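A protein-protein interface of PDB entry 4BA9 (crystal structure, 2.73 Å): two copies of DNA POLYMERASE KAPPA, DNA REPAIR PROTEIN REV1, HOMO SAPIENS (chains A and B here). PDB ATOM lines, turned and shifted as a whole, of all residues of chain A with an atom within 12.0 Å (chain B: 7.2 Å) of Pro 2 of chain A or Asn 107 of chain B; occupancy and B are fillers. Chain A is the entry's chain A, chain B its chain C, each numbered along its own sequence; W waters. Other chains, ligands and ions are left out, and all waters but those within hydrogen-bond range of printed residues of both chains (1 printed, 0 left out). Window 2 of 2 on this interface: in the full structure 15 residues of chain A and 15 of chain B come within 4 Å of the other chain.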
ATOM      1  N   GLY A   1     -25.159   8.821 -23.763  1.00  0.00           N
ATOM      2  CA  GLY A   1     -25.007  10.022 -24.559  1.00  0.00           C
ATOM      3  C   GLY A   1     -23.551  10.343 -24.818  1.00  0.00           C
ATOM      4  O   GLY A   1     -22.681   9.539 -24.462  1.00  0.00           O
ATOM      5  N   PRO A   2     -23.249  11.513 -25.454  1.00  0.00           N
ATOM      6  CA  PRO A   2     -21.842  11.828 -25.795  1.00  0.00           C
ATOM      7  C   PRO A   2     -20.986  11.921 -24.542  1.00  0.00           C
ATOM      8  O   PRO A   2     -21.481  12.283 -23.464  1.00  0.00           O
ATOM      9  CB  PRO A   2     -21.931  13.156 -26.552  1.00  0.00           C
ATOM     10  CG  PRO A   2     -23.344  13.218 -27.051  1.00  0.00           C
ATOM     11  CD  PRO A   2     -24.164  12.552 -25.979  1.00  0.00           C
ATOM     12  N   HIS A   3     -19.707  11.538 -24.682  1.00  0.00           N
ATOM     13  CA  HIS A   3     -18.780  11.457 -23.566  1.00  0.00           C
ATOM     14  C   HIS A   3     -17.325  11.635 -24.014  1.00  0.00           C
ATOM     15  O   HIS A   3     -16.987  11.356 -25.169  1.00  0.00           O
ATOM     16  CB  HIS A   3     -18.944  10.073 -22.901  1.00  0.00           C
ATOM     17  CG  HIS A   3     -18.559   8.919 -23.803  1.00  0.00           C
ATOM     18  ND1 HIS A   3     -19.426   8.453 -24.780  1.00  0.00           N
ATOM     19  CD2 HIS A   3     -17.416   8.182 -23.845  1.00  0.00           C
ATOM     20  CE1 HIS A   3     -18.780   7.472 -25.394  1.00  0.00           C
ATOM     21  NE2 HIS A   3     -17.566   7.274 -24.871  1.00  0.00           N
ATOM     22  N   MET A   4     -16.461  12.032 -23.063  1.00  0.00           N
ATOM     23  CA  MET A   4     -15.021  12.202 -23.245  1.00  0.00           C
ATOM     24  C   MET A   4     -14.271  11.196 -22.391  1.00  0.00           C
ATOM     25  O   MET A   4     -14.726  10.867 -21.283  1.00  0.00           O
ATOM     26  CB  MET A   4     -14.589  13.620 -22.852  1.00  0.00           C
ATOM     27  CG  MET A   4     -15.409  14.699 -23.531  1.00  0.00           C
ATOM     28  SD  MET A   4     -14.679  16.332 -23.506  1.00  0.00           S
ATOM     29  CE  MET A   4     -13.249  16.062 -24.549  1.00  0.00           C
ATOM     30  N   HIS A   5     -13.126  10.701 -22.886  1.00  0.00           N
ATOM     31  CA  HIS A   5     -12.348   9.747 -22.110  1.00  0.00           C
ATOM     32  C   HIS A   5     -11.106  10.410 -21.520  1.00  0.00           C
ATOM     33  O   HIS A   5     -10.250  10.886 -22.251  1.00  0.00           O
ATOM     34  CB  HIS A   5     -11.985   8.500 -22.927  1.00  0.00           C
ATOM     35  CG  HIS A   5     -13.154   7.593 -23.179  1.00  0.00           C
ATOM     36  ND1 HIS A   5     -13.763   6.888 -22.154  1.00  0.00           N
ATOM     37  CD2 HIS A   5     -13.792   7.310 -24.337  1.00  0.00           C
ATOM     38  CE1 HIS A   5     -14.760   6.225 -22.717  1.00  0.00           C
ATOM     39  NE2 HIS A   5     -14.811   6.442 -24.031  1.00  0.00           N
ATOM     40  N   LYS A   6     -11.036  10.457 -20.189  1.00  0.00           N
ATOM     41  CA  LYS A   6      -9.909  10.989 -19.452  1.00  0.00           C
ATOM     42  C   LYS A   6      -9.007   9.799 -19.103  1.00  0.00           C
ATOM     43  O   LYS A   6      -9.319   9.049 -18.180  1.00  0.00           O
ATOM     44  CB  LYS A   6     -10.389  11.758 -18.188  1.00  0.00           C
ATOM     45  CG  LYS A   6     -11.318  12.939 -18.476  1.00  0.00           C
ATOM     46  CD  LYS A   6     -11.116  14.133 -17.547  1.00  0.00           C
ATOM     47  CE  LYS A   6     -11.612  15.384 -18.238  1.00  0.00           C
ATOM     48  NZ  LYS A   6     -11.203  16.628 -17.531  1.00  0.00           N
ATOM     49  N   LYS A   7      -7.919   9.610 -19.857  1.00  0.00           N
ATOM     50  CA  LYS A   7      -6.996   8.488 -19.672  1.00  0.00           C
ATOM     51  C   LYS A   7      -5.784   8.920 -18.871  1.00  0.00           C
ATOM     52  O   LYS A   7      -5.081   9.854 -19.290  1.00  0.00           O
ATOM     53  CB  LYS A   7      -6.523   7.935 -21.031  1.00  0.00           C
ATOM     54  CG  LYS A   7      -7.594   7.272 -21.893  1.00  0.00           C
ATOM     55  CD  LYS A   7      -7.855   8.039 -23.191  1.00  0.00           C
ATOM     56  CE  LYS A   7      -8.781   7.272 -24.113  1.00  0.00           C
ATOM     57  NZ  LYS A   7      -9.316   8.127 -25.207  1.00  0.00           N
ATOM     58  N   GLU B  56     -15.190  19.335 -19.323  1.00  0.00           N
ATOM     59  CA  GLU B  56     -15.985  18.333 -20.010  1.00  0.00           C
ATOM     60  C   GLU B  56     -17.475  18.641 -19.854  1.00  0.00           C
ATOM     61  O   GLU B  56     -18.214  18.552 -20.819  1.00  0.00           O
ATOM     62  CB  GLU B  56     -15.653  16.965 -19.426  1.00  0.00           C
ATOM     63  CG  GLU B  56     -16.321  15.805 -20.144  1.00  0.00           C
ATOM     64  CD  GLU B  56     -16.199  14.451 -19.480  1.00  0.00           C
ATOM     65  OE1 GLU B  56     -15.298  14.281 -18.626  1.00  0.00           O
ATOM     66  OE2 GLU B  56     -16.996  13.550 -19.833  1.00  0.00           O
ATOM     67  N   LEU B  60     -19.908  19.336 -23.004  1.00  0.00           N
ATOM     68  CA  LEU B  60     -21.082  18.484 -23.190  1.00  0.00           C
ATOM     69  C   LEU B  60     -22.387  19.260 -23.099  1.00  0.00           C
ATOM     70  O   LEU B  60     -23.352  18.875 -23.756  1.00  0.00           O
ATOM     71  CB  LEU B  60     -21.078  17.292 -22.222  1.00  0.00           C
ATOM     72  CG  LEU B  60     -19.943  16.303 -22.419  1.00  0.00           C
ATOM     73  CD1 LEU B  60     -19.810  15.421 -21.235  1.00  0.00           C
ATOM     74  CD2 LEU B  60     -20.083  15.522 -23.728  1.00  0.00           C
ATOM     75  N   VAL B  63     -22.713  20.692 -26.671  1.00  0.00           N
ATOM     76  CA  VAL B  63     -23.132  19.570 -27.546  1.00  0.00           C
ATOM     77  C   VAL B  63     -24.644  19.327 -27.363  1.00  0.00           C
ATOM     78  O   VAL B  63     -25.350  19.253 -28.357  1.00  0.00           O
ATOM     79  CB  VAL B  63     -22.299  18.278 -27.313  1.00  0.00           C
ATOM     80  CG1 VAL B  63     -22.875  17.100 -28.083  1.00  0.00           C
ATOM     81  CG2 VAL B  63     -20.848  18.476 -27.709  1.00  0.00           C
ATOM     82  N   LYS B  64     -25.144  19.283 -26.109  1.00  0.00           N
ATOM     83  CA  LYS B  64     -26.582  19.073 -25.879  1.00  0.00           C
ATOM     84  C   LYS B  64     -27.412  20.194 -26.502  1.00  0.00           C
ATOM     85  O   LYS B  64     -28.414  19.900 -27.151  1.00  0.00           O
ATOM     86  CB  LYS B  64     -26.934  18.922 -24.388  1.00  0.00           C
ATOM     87  CG  LYS B  64     -28.376  18.437 -24.216  1.00  0.00           C
ATOM     88  CD  LYS B  64     -28.848  18.423 -22.778  1.00  0.00           C
ATOM     89  CE  LYS B  64     -30.289  17.993 -22.681  1.00  0.00           C
ATOM     90  NZ  LYS B  64     -31.221  19.114 -22.969  1.00  0.00           N
ATOM     91  N   THR B  67     -27.555  19.682 -30.251  1.00  0.00           N
ATOM     92  CA  THR B  67     -28.391  18.539 -30.654  1.00  0.00           C
ATOM     93  C   THR B  67     -29.861  18.830 -30.364  1.00  0.00           C
ATOM     94  O   THR B  67     -30.732  18.253 -31.032  1.00  0.00           O
ATOM     95  CB  THR B  67     -27.940  17.222 -30.012  1.00  0.00           C
ATOM     96  OG1 THR B  67     -28.268  17.225 -28.603  1.00  0.00           O
ATOM     97  CG2 THR B  67     -26.490  16.907 -30.287  1.00  0.00           C
ATOM     98  N   ILE B  70     -31.053  20.686 -33.396  1.00  0.00           N
ATOM     99  CA  ILE B  70     -31.294  19.682 -34.436  1.00  0.00           C
ATOM    100  C   ILE B  70     -32.687  19.039 -34.179  1.00  0.00           C
ATOM    101  O   ILE B  70     -33.489  18.930 -35.103  1.00  0.00           O
ATOM    102  CB  ILE B  70     -30.135  18.631 -34.500  1.00  0.00           C
ATOM    103  CG1 ILE B  70     -28.790  19.268 -34.903  1.00  0.00           C
ATOM    104  CG2 ILE B  70     -30.464  17.496 -35.479  1.00  0.00           C
ATOM    105  CD1 ILE B  70     -27.534  18.348 -34.766  1.00  0.00           C
ATOM    106  N   PHE B 101     -13.330  22.001 -29.947  1.00  0.00           N
ATOM    107  CA  PHE B 101     -14.116  22.256 -31.149  1.00  0.00           C
ATOM    108  C   PHE B 101     -14.290  20.956 -31.928  1.00  0.00           C
ATOM    109  O   PHE B 101     -15.431  20.635 -32.262  1.00  0.00           O
ATOM    110  CB  PHE B 101     -13.513  23.365 -32.054  1.00  0.00           C
ATOM    111  CG  PHE B 101     -14.295  23.533 -33.333  1.00  0.00           C
ATOM    112  CD1 PHE B 101     -15.579  24.083 -33.315  1.00  0.00           C
ATOM    113  CD2 PHE B 101     -13.801  23.044 -34.537  1.00  0.00           C
ATOM    114  CE1 PHE B 101     -16.344  24.145 -34.476  1.00  0.00           C
ATOM    115  CE2 PHE B 101     -14.564  23.113 -35.696  1.00  0.00           C
ATOM    116  CZ  PHE B 101     -15.832  23.663 -35.656  1.00  0.00           C
ATOM    117  N   ASP B 102     -13.185  20.210 -32.203  1.00  0.00           N
ATOM    118  CA  ASP B 102     -13.255  18.939 -32.927  1.00  0.00           C
ATOM    119  C   ASP B 102     -14.310  18.037 -32.296  1.00  0.00           C
ATOM    120  O   ASP B 102     -15.222  17.624 -33.000  1.00  0.00           O
ATOM    121  CB  ASP B 102     -11.900  18.226 -33.005  1.00  0.00           C
ATOM    122  CG  ASP B 102     -10.840  18.918 -33.849  1.00  0.00           C
ATOM    123  OD1 ASP B 102     -11.211  19.725 -34.745  1.00  0.00           O
ATOM    124  OD2 ASP B 102      -9.643  18.636 -33.637  1.00  0.00           O
ATOM    125  N   PHE B 103     -14.266  17.854 -30.961  1.00  0.00           N
ATOM    126  CA  PHE B 103     -15.236  17.047 -30.236  1.00  0.00           C
ATOM    127  C   PHE B 103     -16.677  17.551 -30.460  1.00  0.00           C
ATOM    128  O   PHE B 103     -17.559  16.737 -30.744  1.00  0.00           O
ATOM    129  CB  PHE B 103     -14.907  16.989 -28.726  1.00  0.00           C
ATOM    130  CG  PHE B 103     -15.877  16.123 -27.949  1.00  0.00           C
ATOM    131  CD1 PHE B 103     -15.649  14.759 -27.796  1.00  0.00           C
ATOM    132  CD2 PHE B 103     -17.038  16.666 -27.403  1.00  0.00           C
ATOM    133  CE1 PHE B 103     -16.555  13.959 -27.105  1.00  0.00           C
ATOM    134  CE2 PHE B 103     -17.946  15.864 -26.706  1.00  0.00           C
ATOM    135  CZ  PHE B 103     -17.702  14.517 -26.567  1.00  0.00           C
ATOM    136  N   ILE B 104     -16.920  18.867 -30.309  1.00  0.00           N
ATOM    137  CA  ILE B 104     -18.266  19.420 -30.483  1.00  0.00           C
ATOM    138  C   ILE B 104     -18.740  19.139 -31.917  1.00  0.00           C
ATOM    139  O   ILE B 104     -19.813  18.580 -32.103  1.00  0.00           O
ATOM    140  CB  ILE B 104     -18.355  20.938 -30.112  1.00  0.00           C
ATOM    141  CG1 ILE B 104     -18.003  21.175 -28.626  1.00  0.00           C
ATOM    142  CG2 ILE B 104     -19.762  21.514 -30.423  1.00  0.00           C
ATOM    143  CD1 ILE B 104     -17.710  22.589 -28.254  1.00  0.00           C
ATOM    144  N   LEU B 105     -17.906  19.488 -32.915  1.00  0.00           N
ATOM    145  CA  LEU B 105     -18.193  19.309 -34.334  1.00  0.00           C
ATOM    146  C   LEU B 105     -18.463  17.841 -34.648  1.00  0.00           C
ATOM    147  O   LEU B 105     -19.562  17.543 -35.110  1.00  0.00           O
ATOM    148  CB  LEU B 105     -17.032  19.853 -35.204  1.00  0.00           C
ATOM    149  CG  LEU B 105     -17.148  19.655 -36.715  1.00  0.00           C
ATOM    150  CD1 LEU B 105     -18.237  20.538 -37.289  1.00  0.00           C
ATOM    151  CD2 LEU B 105     -15.821  19.852 -37.403  1.00  0.00           C
ATOM    152  N   ASP B 106     -17.495  16.938 -34.369  1.00  0.00           N
ATOM    153  CA  ASP B 106     -17.616  15.498 -34.622  1.00  0.00           C
ATOM    154  C   ASP B 106     -18.916  14.900 -34.029  1.00  0.00           C
ATOM    155  O   ASP B 106     -19.580  14.135 -34.714  1.00  0.00           O
ATOM    156  CB  ASP B 106     -16.387  14.736 -34.100  1.00  0.00           C
ATOM    157  CG  ASP B 106     -15.055  15.072 -34.782  1.00  0.00           C
ATOM    158  OD1 ASP B 106     -15.058  15.891 -35.747  1.00  0.00           O
ATOM    159  OD2 ASP B 106     -14.006  14.534 -34.342  1.00  0.00           O
ATOM    160  N   ASN B 107     -19.312  15.308 -32.825  1.00  0.00           N
ATOM    161  CA  ASN B 107     -20.522  14.807 -32.182  1.00  0.00           C
ATOM    162  C   ASN B 107     -21.798  15.392 -32.772  1.00  0.00           C
ATOM    163  O   ASN B 107     -22.850  14.757 -32.682  1.00  0.00           O
ATOM    164  CB  ASN B 107     -20.456  15.071 -30.651  1.00  0.00           C
ATOM    165  CG  ASN B 107     -19.630  14.024 -29.953  1.00  0.00           C
ATOM    166  OD1 ASN B 107     -20.166  13.073 -29.406  1.00  0.00           O
ATOM    167  ND2 ASN B 107     -18.307  14.090 -30.071  1.00  0.00           N
ATOM    168  N   VAL B 108     -21.702  16.596 -33.360  1.00  0.00           N
ATOM    169  CA  VAL B 108     -22.842  17.281 -33.985  1.00  0.00           C
ATOM    170  C   VAL B 108     -23.052  16.697 -35.381  1.00  0.00           C
ATOM    171  O   VAL B 108     -24.192  16.415 -35.766  1.00  0.00           O
ATOM    172  CB  VAL B 108     -22.657  18.838 -34.006  1.00  0.00           C
ATOM    173  CG1 VAL B 108     -23.693  19.527 -34.881  1.00  0.00           C
ATOM    174  CG2 VAL B 108     -22.739  19.417 -32.616  1.00  0.00           C
ATOM    175  N   GLN B 109     -21.944  16.503 -36.118  1.00  0.00           N
ATOM    176  CA  GLN B 109     -21.932  15.954 -37.468  1.00  0.00           C
ATOM    177  C   GLN B 109     -22.630  14.609 -37.524  1.00  0.00           C
ATOM    178  O   GLN B 109     -23.422  14.410 -38.432  1.00  0.00           O
ATOM    179  CB  GLN B 109     -20.507  15.820 -38.005  1.00  0.00           C
ATOM    180  CG  GLN B 109     -19.963  17.098 -38.606  1.00  0.00           C
ATOM    181  CD  GLN B 109     -20.848  17.789 -39.630  1.00  0.00           C
ATOM    182  OE1 GLN B 109     -20.965  17.340 -40.771  1.00  0.00           O
ATOM    183  NE2 GLN B 109     -21.476  18.884 -39.246  1.00  0.00           N
ATOM    184  N   VAL B 110     -22.365  13.720 -36.536  1.00  0.00           N
ATOM    185  CA  VAL B 110     -22.956  12.397 -36.369  1.00  0.00           C
ATOM    186  C   VAL B 110     -24.493  12.508 -36.390  1.00  0.00           C
ATOM    187  O   VAL B 110     -25.132  11.785 -37.155  1.00  0.00           O
ATOM    188  CB  VAL B 110     -22.440  11.739 -35.045  1.00  0.00           C
ATOM    189  CG1 VAL B 110     -23.315  10.580 -34.594  1.00  0.00           C
ATOM    190  CG2 VAL B 110     -20.996  11.280 -35.187  1.00  0.00           C
ATOM    191  N   VAL B 111     -25.068  13.419 -35.581  1.00  0.00           N
ATOM    192  CA  VAL B 111     -26.521  13.608 -35.478  1.00  0.00           C
ATOM    193  C   VAL B 111     -27.065  14.214 -36.801  1.00  0.00           C
ATOM    194  O   VAL B 111     -28.168  13.861 -37.246  1.00  0.00           O
ATOM    195  CB  VAL B 111     -26.904  14.458 -34.218  1.00  0.00           C
ATOM    196  CG1 VAL B 111     -28.404  14.460 -34.000  1.00  0.00           C
ATOM    197  CG2 VAL B 111     -26.217  13.936 -32.971  1.00  0.00           C
ATOM    198  N   LEU B 112     -26.275  15.103 -37.431  1.00  0.00           N
ATOM    199  CA  LEU B 112     -26.669  15.749 -38.687  1.00  0.00           C
ATOM    200  C   LEU B 112     -26.700  14.748 -39.851  1.00  0.00           C
ATOM    201  O   LEU B 112     -27.616  14.790 -40.679  1.00  0.00           O
ATOM    202  CB  LEU B 112     -25.711  16.904 -39.027  1.00  0.00           C
ATOM    203  CG  LEU B 112     -25.893  18.214 -38.260  1.00  0.00           C
ATOM    204  CD1 LEU B 112     -24.787  19.179 -38.628  1.00  0.00           C
ATOM    205  CD2 LEU B 112     -27.287  18.826 -38.505  1.00  0.00           C
HETATM  206  O   HOH W   1     -19.071  10.842 -27.519  1.00  0.00           O
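The backbone carbonyl oxygen (O) of Gly 1 of chain A lies close to a ring nitrogen (ND1) of His 3 of chain A (3.4 Å).
The backbone carbonyl oxygen (O) of Phe 103 of chain B sits at hydrogen-bond distance from the side-chain amide nitrogen (ND2) of Asn 107 of chain B (2.8 Å).
Among the printed residues, merely in contact across the chains: His 3 of chain A with Phe 103 of chain B, Pro 2 of chain A with Asn 107 of chain B, Pro 2 of chain A with Leu 60 of chain B, Met 4 of chain A with Glu 56 of chain B, Met 4 of chain A with Phe 103 of chain B and Lys 6 of chain A with Glu 56 of chain B.
Gly 1 of chain A touches none of the printed residues of chain B.
Of chain B, only Leu 60 (3.5 Å) and Asn 107 (3.4 Å) come within 4 Å of Pro 2 of chain A.
Of the printed residues of chain B, His 3 of chain A touches Phe 103 (3.3 Å).
Printed residues of chain B within 4 Å of Met 4 of chain A: Glu 56 (3.6 Å) and Phe 103 (3.8 Å).
His 5 of chain A touches none of the printed residues of chain B.
Printed residues of chain B within 4 Å of Lys 6 of chain A: Glu 56 (3.9 Å).
Printed residues of chain A within 4 Å of Glu 56 of chain B: Met 4 and Lys 6.
Leu 60 of chain B touches just one residue of chain A: Pro 2.
No residue of chain A comes within 4 Å of Val 63 of chain B.
Of chain A, only His 3 (3.3 Å) and Met 4 (3.8 Å) come within 4 Å of Phe 103 of chain B.
No residue of chain A comes within 4 Å of Leu 105 of chain B.
Asn 107 of chain B touches just one residue of chain A: Pro 2 (3.4 Å).
No residue of chain A comes within 4 Å of Val 108 of chain B.
No residue of chain A comes within 4 Å of Val 110 of chain B.
No residue of chain A comes within 4 Å of Val 111 of chain B.
The nearest residue of chain B that does not touch Pro 2 of chain A is Val 63 of chain B (4.04 Å).
The nearest residue of chain A that does not touch Asn 107 of chain B is His 3 of chain A (5.0 Å).
The nearest printed residue of chain B that does not touch Lys 6 of chain A is Leu 60 of chain B (8.7 Å).
Printed residues of chain B that touch a printed residue of chain A: Glu 56, Leu 60, Phe 103 and Asn 107.
Hydrophobic or aromatic side chains of chain B that line the printed part of chain A: Leu 60 and Phe 103.
No position is printed for both chains.
Of the 6 pairs that touch across the chains among the printed residues, none has its exchanged pair printed and touching as well.
Water W1 lies within hydrogen-bond range of N of His 3 of chain A and OD1 of Asn 107 of chain B.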
